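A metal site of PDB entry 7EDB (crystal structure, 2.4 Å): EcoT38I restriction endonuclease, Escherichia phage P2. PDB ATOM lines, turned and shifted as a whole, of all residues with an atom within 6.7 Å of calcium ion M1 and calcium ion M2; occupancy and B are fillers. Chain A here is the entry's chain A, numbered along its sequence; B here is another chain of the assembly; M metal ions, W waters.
The backbone carbonyl oxygen of Ile 244 is in hydrogen-bond range of the backbone NH of Asp 231. OE1 of Glu 245 lies close to NZ of Lys 247, at 2.8 Å. O5' of DT 9 of chain B sits at hydrogen-bond distance from N of Gly 223 (2.9 Å). OP2 of DC 10 of chain B is in salt-bridge range of the side-chain amino group (NZ) of Lys 247, at 3.9 Å. OP1 of DT 9 of chain B is in salt-bridge range of the side-chain amino group of Lys 262 (2.8 Å).
Within 4 Å of calcium ion M1: Asp 231, Glu 245, Val 246 and DC 10 of chain B.
Within 4 Å of calcium ion M2: Asp 231, DT 9 of chain B and DC 10 of chain B.
Calcium ion M1 is bound by OP1 of DC 10 of chain B (2.2 Å), the backbone carbonyl oxygen of Val 246 (2.3 Å), the side-chain carboxylate of Asp 231 (2.3 Å), the side-chain carboxylate of Glu 245 (2.3 Å), water W5 (2.3 Å) and water W1 (2.4 Å). Calcium ion M1 has six donor atoms within binding distance. Slightly farther from calcium ion M1 lies OD1 of Asp 231 (3.1 Å).
Calcium ion M2 is bound by water W2 (2.3 Å), the side-chain carboxylate (OD1) of Asp 231 (2.4 Å), water W6 (2.4 Å), water W3 (2.5 Å), water W4 (2.5 Å), OP1 of DC 10 of chain B (2.5 Å) and O3' of DT 9 of chain B (2.6 Å). Calcium ion M2 has seven donor atoms within binding distance.
Water W5 lies within hydrogen-bond range of OP2 of DT 11 of chain B (2.7 Å), OP2 of DC 10 of chain B (3.1 Å) and the side-chain amino group (NZ) of Lys 247 (3.5 Å). Water W4 lies within hydrogen-bond range of the side-chain amino group (NZ) of Lys 262 and the side-chain carboxylate (OE2) of Glu 245. Water W6 lies within hydrogen-bond range of the side-chain carboxylate (OE1) of Glu 228 and the backbone carbonyl oxygen (O) of Gln 221.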
ATOM      1  N   PRO A 218      35.045  -6.223 -12.284  1.00  0.00           N
ATOM      2  CA  PRO A 218      34.301  -5.790 -13.487  1.00  0.00           C
ATOM      3  C   PRO A 218      32.948  -6.489 -13.572  1.00  0.00           C
ATOM      4  O   PRO A 218      32.856  -7.711 -13.443  1.00  0.00           O
ATOM      5  CB  PRO A 218      35.224  -6.205 -14.639  1.00  0.00           C
ATOM      6  CG  PRO A 218      36.614  -6.229 -14.021  1.00  0.00           C
ATOM      7  CD  PRO A 218      36.431  -6.638 -12.585  1.00  0.00           C
ATOM      8  N   VAL A 219      31.881  -5.703 -13.771  1.00  0.00           N
ATOM      9  CA  VAL A 219      30.546  -6.278 -13.640  1.00  0.00           C
ATOM     10  C   VAL A 219      30.260  -7.335 -14.699  1.00  0.00           C
ATOM     11  O   VAL A 219      29.377  -8.167 -14.495  1.00  0.00           O
ATOM     12  CB  VAL A 219      29.429  -5.213 -13.654  1.00  0.00           C
ATOM     13  CG1 VAL A 219      29.692  -4.140 -12.609  1.00  0.00           C
ATOM     14  CG2 VAL A 219      29.230  -4.617 -15.051  1.00  0.00           C
ATOM     15  N   GLN A 221      32.488  -9.608 -15.657  1.00  0.00           N
ATOM     16  CA  GLN A 221      33.247 -10.801 -15.345  1.00  0.00           C
ATOM     17  C   GLN A 221      32.303 -11.882 -14.793  1.00  0.00           C
ATOM     18  O   GLN A 221      31.450 -11.608 -13.951  1.00  0.00           O
ATOM     19  CB  GLN A 221      34.336 -10.483 -14.329  1.00  0.00           C
ATOM     20  CG  GLN A 221      35.098 -11.707 -13.866  1.00  0.00           C
ATOM     21  CD  GLN A 221      36.268 -11.342 -12.968  1.00  0.00           C
ATOM     22  OE1 GLN A 221      37.322 -10.952 -13.456  1.00  0.00           O
ATOM     23  NE2 GLN A 221      36.066 -11.445 -11.650  1.00  0.00           N
ATOM     24  N   ALA A 222      32.445 -13.094 -15.308  1.00  0.00           N
ATOM     25  CA  ALA A 222      31.487 -14.161 -15.071  1.00  0.00           C
ATOM     26  C   ALA A 222      31.761 -14.884 -13.756  1.00  0.00           C
ATOM     27  O   ALA A 222      32.906 -14.971 -13.293  1.00  0.00           O
ATOM     28  CB  ALA A 222      31.505 -15.156 -16.236  1.00  0.00           C
ATOM     29  N   GLY A 223      30.696 -15.412 -13.157  1.00  0.00           N
ATOM     30  CA  GLY A 223      30.833 -16.199 -11.941  1.00  0.00           C
ATOM     31  C   GLY A 223      31.659 -17.470 -12.108  1.00  0.00           C
ATOM     32  O   GLY A 223      32.101 -18.044 -11.117  1.00  0.00           O
ATOM     33  N   GLU A 228      36.882 -14.331  -8.754  1.00  0.00           N
ATOM     34  CA  GLU A 228      35.836 -13.751  -7.937  1.00  0.00           C
ATOM     35  C   GLU A 228      35.036 -14.853  -7.255  1.00  0.00           C
ATOM     36  O   GLU A 228      35.026 -16.006  -7.707  1.00  0.00           O
ATOM     37  CB  GLU A 228      34.888 -12.887  -8.776  1.00  0.00           C
ATOM     38  CG  GLU A 228      33.969 -13.714  -9.711  1.00  0.00           C
ATOM     39  CD  GLU A 228      32.944 -12.845 -10.449  1.00  0.00           C
ATOM     40  OE1 GLU A 228      31.727 -13.133 -10.336  1.00  0.00           O
ATOM     41  OE2 GLU A 228      33.354 -11.867 -11.124  1.00  0.00           O
ATOM     42  N   ILE A 229      34.336 -14.476  -6.191  1.00  0.00           N
ATOM     43  CA  ILE A 229      33.244 -15.307  -5.701  1.00  0.00           C
ATOM     44  C   ILE A 229      31.929 -14.650  -6.114  1.00  0.00           C
ATOM     45  O   ILE A 229      31.192 -15.199  -6.928  1.00  0.00           O
ATOM     46  CB  ILE A 229      33.373 -15.555  -4.187  1.00  0.00           C
ATOM     47  CG1 ILE A 229      34.627 -16.385  -3.923  1.00  0.00           C
ATOM     48  CG2 ILE A 229      32.182 -16.343  -3.658  1.00  0.00           C
ATOM     49  CD1 ILE A 229      35.555 -15.764  -2.971  1.00  0.00           C
ATOM     50  N   LEU A 230      31.639 -13.455  -5.596  1.00  0.00           N
ATOM     51  CA  LEU A 230      30.447 -12.750  -6.085  1.00  0.00           C
ATOM     52  C   LEU A 230      30.822 -11.378  -6.657  1.00  0.00           C
ATOM     53  O   LEU A 230      31.931 -11.218  -7.172  1.00  0.00           O
ATOM     54  CB  LEU A 230      29.403 -12.629  -4.967  1.00  0.00           C
ATOM     55  CG  LEU A 230      28.797 -13.942  -4.437  1.00  0.00           C
ATOM     56  CD1 LEU A 230      27.691 -13.663  -3.400  1.00  0.00           C
ATOM     57  CD2 LEU A 230      28.276 -14.837  -5.567  1.00  0.00           C
ATOM     58  N   ASP A 231      29.923 -10.393  -6.587  1.00  0.00           N
ATOM     59  CA  ASP A 231      30.188  -9.083  -7.191  1.00  0.00           C
ATOM     60  C   ASP A 231      31.326  -8.364  -6.485  1.00  0.00           C
ATOM     61  O   ASP A 231      32.182  -7.761  -7.130  1.00  0.00           O
ATOM     62  CB  ASP A 231      28.941  -8.204  -7.162  1.00  0.00           C
ATOM     63  CG  ASP A 231      27.872  -8.726  -8.070  1.00  0.00           C
ATOM     64  OD1 ASP A 231      28.241  -9.371  -9.064  1.00  0.00           O
ATOM     65  OD2 ASP A 231      26.675  -8.512  -7.774  1.00  0.00           O
ATOM     66  N   ILE A 244      29.317 -10.046  -1.580  1.00  0.00           N
ATOM     67  CA  ILE A 244      28.125  -9.275  -1.855  1.00  0.00           C
ATOM     68  C   ILE A 244      27.676  -9.562  -3.277  1.00  0.00           C
ATOM     69  O   ILE A 244      28.487  -9.519  -4.209  1.00  0.00           O
ATOM     70  CB  ILE A 244      28.361  -7.754  -1.655  1.00  0.00           C
ATOM     71  CG1 ILE A 244      28.571  -7.414  -0.180  1.00  0.00           C
ATOM     72  CG2 ILE A 244      27.196  -6.939  -2.180  1.00  0.00           C
ATOM     73  CD1 ILE A 244      29.978  -7.343   0.207  1.00  0.00           C
ATOM     74  N   GLU A 245      26.396  -9.860  -3.450  1.00  0.00           N
ATOM     75  CA  GLU A 245      25.741  -9.890  -4.755  1.00  0.00           C
ATOM     76  C   GLU A 245      24.839  -8.669  -4.864  1.00  0.00           C
ATOM     77  O   GLU A 245      23.967  -8.464  -4.016  1.00  0.00           O
ATOM     78  CB  GLU A 245      24.922 -11.162  -4.924  1.00  0.00           C
ATOM     79  CG  GLU A 245      24.069 -11.185  -6.192  1.00  0.00           C
ATOM     80  CD  GLU A 245      24.896 -11.282  -7.483  1.00  0.00           C
ATOM     81  OE1 GLU A 245      24.458 -10.696  -8.505  1.00  0.00           O
ATOM     82  OE2 GLU A 245      25.958 -11.952  -7.487  1.00  0.00           O
ATOM     83  N   VAL A 246      25.031  -7.865  -5.898  1.00  0.00           N
ATOM     84  CA  VAL A 246      24.173  -6.710  -6.170  1.00  0.00           C
ATOM     85  C   VAL A 246      23.253  -7.055  -7.322  1.00  0.00           C
ATOM     86  O   VAL A 246      23.695  -7.610  -8.323  1.00  0.00           O
ATOM     87  CB  VAL A 246      25.000  -5.444  -6.500  1.00  0.00           C
ATOM     88  CG1 VAL A 246      24.091  -4.236  -6.547  1.00  0.00           C
ATOM     89  CG2 VAL A 246      26.096  -5.228  -5.486  1.00  0.00           C
ATOM     90  N   LYS A 247      21.975  -6.735  -7.201  1.00  0.00           N
ATOM     91  CA  LYS A 247      21.026  -6.856  -8.302  1.00  0.00           C
ATOM     92  C   LYS A 247      20.366  -5.510  -8.548  1.00  0.00           C
ATOM     93  O   LYS A 247      19.709  -4.966  -7.652  1.00  0.00           O
ATOM     94  CB  LYS A 247      19.967  -7.921  -8.009  1.00  0.00           C
ATOM     95  CG  LYS A 247      20.507  -9.310  -7.759  1.00  0.00           C
ATOM     96  CD  LYS A 247      20.798 -10.033  -9.063  1.00  0.00           C
ATOM     97  CE  LYS A 247      21.233 -11.468  -8.793  1.00  0.00           C
ATOM     98  NZ  LYS A 247      22.239 -11.927  -9.795  1.00  0.00           N
ATOM     99  N   ASP A 248      20.522  -4.973  -9.747  1.00  0.00           N
ATOM    100  CA  ASP A 248      19.815  -3.761 -10.152  1.00  0.00           C
ATOM    101  C   ASP A 248      18.876  -4.103 -11.299  1.00  0.00           C
ATOM    102  O   ASP A 248      18.767  -3.377 -12.290  1.00  0.00           O
ATOM    103  CB  ASP A 248      20.763  -2.623 -10.513  1.00  0.00           C
ATOM    104  CG  ASP A 248      20.071  -1.233 -10.458  1.00  0.00           C
ATOM    105  OD1 ASP A 248      18.924  -1.162  -9.972  1.00  0.00           O
ATOM    106  OD2 ASP A 248      20.661  -0.217 -10.892  1.00  0.00           O
ATOM    107  N   LYS A 262      27.429 -20.369  -5.246  1.00  0.00           N
ATOM    108  CA  LYS A 262      28.807 -19.991  -5.553  1.00  0.00           C
ATOM    109  C   LYS A 262      29.569 -19.682  -4.264  1.00  0.00           C
ATOM    110  O   LYS A 262      30.728 -20.094  -4.108  1.00  0.00           O
ATOM    111  CB  LYS A 262      28.818 -18.798  -6.523  1.00  0.00           C
ATOM    112  CG  LYS A 262      28.499 -19.214  -7.980  1.00  0.00           C
ATOM    113  CD  LYS A 262      28.774 -18.094  -9.062  1.00  0.00           C
ATOM    114  CE  LYS A 262      27.611 -17.068  -9.151  1.00  0.00           C
ATOM    115  NZ  LYS A 262      27.771 -15.850 -10.081  1.00  0.00           N
ATOM    116  P    DT B   9      27.372 -16.713 -13.923  1.00  0.00           P
ATOM    117  OP1  DT B   9      27.658 -17.219 -12.557  1.00  0.00           O
ATOM    118  OP2  DT B   9      25.974 -16.758 -14.413  1.00  0.00           O
ATOM    119  O5'  DT B   9      27.928 -15.221 -14.009  1.00  0.00           O
ATOM    120  C5'  DT B   9      27.066 -14.123 -14.183  1.00  0.00           C
ATOM    121  C4'  DT B   9      27.893 -12.874 -14.421  1.00  0.00           C
ATOM    122  O4'  DT B   9      28.518 -12.958 -15.735  1.00  0.00           O
ATOM    123  C3'  DT B   9      27.098 -11.584 -14.435  1.00  0.00           C
ATOM    124  O3'  DT B   9      27.037 -11.058 -13.144  1.00  0.00           O
ATOM    125  C2'  DT B   9      27.932 -10.704 -15.355  1.00  0.00           C
ATOM    126  C1'  DT B   9      28.419 -11.720 -16.385  1.00  0.00           C
ATOM    127  N1   DT B   9      27.535 -11.865 -17.586  1.00  0.00           N
ATOM    128  C2   DT B   9      27.491 -10.838 -18.519  1.00  0.00           C
ATOM    129  O2   DT B   9      28.129  -9.819 -18.396  1.00  0.00           O
ATOM    130  N3   DT B   9      26.681 -11.064 -19.591  1.00  0.00           N
ATOM    131  C4   DT B   9      25.916 -12.176 -19.839  1.00  0.00           C
ATOM    132  O4   DT B   9      25.214 -12.272 -20.840  1.00  0.00           O
ATOM    133  C5   DT B   9      25.978 -13.211 -18.828  1.00  0.00           C
ATOM    134  C7   DT B   9      25.167 -14.465 -18.977  1.00  0.00           C
ATOM    135  C6   DT B   9      26.784 -13.015 -17.758  1.00  0.00           C
ATOM    136  P    DC B  10      25.705 -10.353 -12.618  1.00  0.00           P
ATOM    137  OP1  DC B  10      26.045  -9.818 -11.309  1.00  0.00           O
ATOM    138  OP2  DC B  10      24.528 -11.220 -12.856  1.00  0.00           O
ATOM    139  O5'  DC B  10      25.450  -9.098 -13.601  1.00  0.00           O
ATOM    140  C5'  DC B  10      26.251  -7.942 -13.481  1.00  0.00           C
ATOM    141  C4'  DC B  10      25.875  -6.956 -14.557  1.00  0.00           C
ATOM    142  O4'  DC B  10      26.283  -7.476 -15.836  1.00  0.00           O
ATOM    143  C3'  DC B  10      24.385  -6.703 -14.745  1.00  0.00           C
ATOM    144  O3'  DC B  10      23.900  -5.774 -13.786  1.00  0.00           O
ATOM    145  C2'  DC B  10      24.385  -6.108 -16.138  1.00  0.00           C
ATOM    146  C1'  DC B  10      25.382  -7.043 -16.837  1.00  0.00           C
ATOM    147  N1   DC B  10      24.681  -8.220 -17.458  1.00  0.00           N
ATOM    148  C2   DC B  10      24.140  -8.067 -18.739  1.00  0.00           C
ATOM    149  O2   DC B  10      24.312  -6.996 -19.337  1.00  0.00           O
ATOM    150  N3   DC B  10      23.481  -9.112 -19.305  1.00  0.00           N
ATOM    151  C4   DC B  10      23.321 -10.251 -18.624  1.00  0.00           C
ATOM    152  N4   DC B  10      22.642 -11.241 -19.220  1.00  0.00           N
ATOM    153  C5   DC B  10      23.849 -10.426 -17.301  1.00  0.00           C
ATOM    154  C6   DC B  10      24.512  -9.390 -16.758  1.00  0.00           C
ATOM    155  P    DT B  11      22.420  -5.935 -13.173  1.00  0.00           P
ATOM    156  OP1  DT B  11      22.315  -4.908 -12.119  1.00  0.00           O
ATOM    157  OP2  DT B  11      22.168  -7.350 -12.831  1.00  0.00           O
ATOM    158  O5'  DT B  11      21.429  -5.615 -14.392  1.00  0.00           O
ATOM    159  C5'  DT B  11      21.181  -4.272 -14.778  1.00  0.00           C
ATOM    160  C4'  DT B  11      21.055  -4.145 -16.295  1.00  0.00           C
ATOM    161  O4'  DT B  11      20.252  -5.221 -16.840  1.00  0.00           O
ATOM    162  C3'  DT B  11      20.396  -2.844 -16.764  1.00  0.00           C
ATOM    163  O3'  DT B  11      21.310  -2.098 -17.541  1.00  0.00           O
ATOM    164  C2'  DT B  11      19.169  -3.308 -17.586  1.00  0.00           C
ATOM    165  C1'  DT B  11      19.568  -4.721 -17.967  1.00  0.00           C
ATOM    166  N1   DT B  11      18.384  -5.621 -18.299  1.00  0.00           N
ATOM    167  C2   DT B  11      18.333  -6.236 -19.531  1.00  0.00           C
ATOM    168  O2   DT B  11      19.200  -6.107 -20.374  1.00  0.00           O
ATOM    169  N3   DT B  11      17.249  -7.018 -19.740  1.00  0.00           N
ATOM    170  C4   DT B  11      16.189  -7.242 -18.872  1.00  0.00           C
ATOM    171  O4   DT B  11      15.245  -7.989 -19.162  1.00  0.00           O
ATOM    172  C5   DT B  11      16.290  -6.556 -17.603  1.00  0.00           C
ATOM    173  C7   DT B  11      15.196  -6.714 -16.575  1.00  0.00           C
ATOM    174  C6   DT B  11      17.365  -5.783 -17.383  1.00  0.00           C
HETATM  175 CA    CA M   1      25.237  -8.767  -9.506  1.00  0.00          CA
HETATM  176 CA    CA M   2      28.223 -10.970 -10.792  1.00  0.00          CA
HETATM  177  O   HOH W   1      25.973  -6.599 -10.357  1.00  0.00           O
HETATM  178  O   HOH W   2      28.254 -12.433  -8.972  1.00  0.00           O
HETATM  179  O   HOH W   3      29.466  -9.155 -11.915  1.00  0.00           O
HETATM  180  O   HOH W   4      26.818 -13.027 -10.638  1.00  0.00           O
HETATM  181  O   HOH W   5      23.444  -8.923 -11.009  1.00  0.00           O
HETATM  182  O   HOH W   6      30.033 -12.207 -11.860  1.00  0.00           O
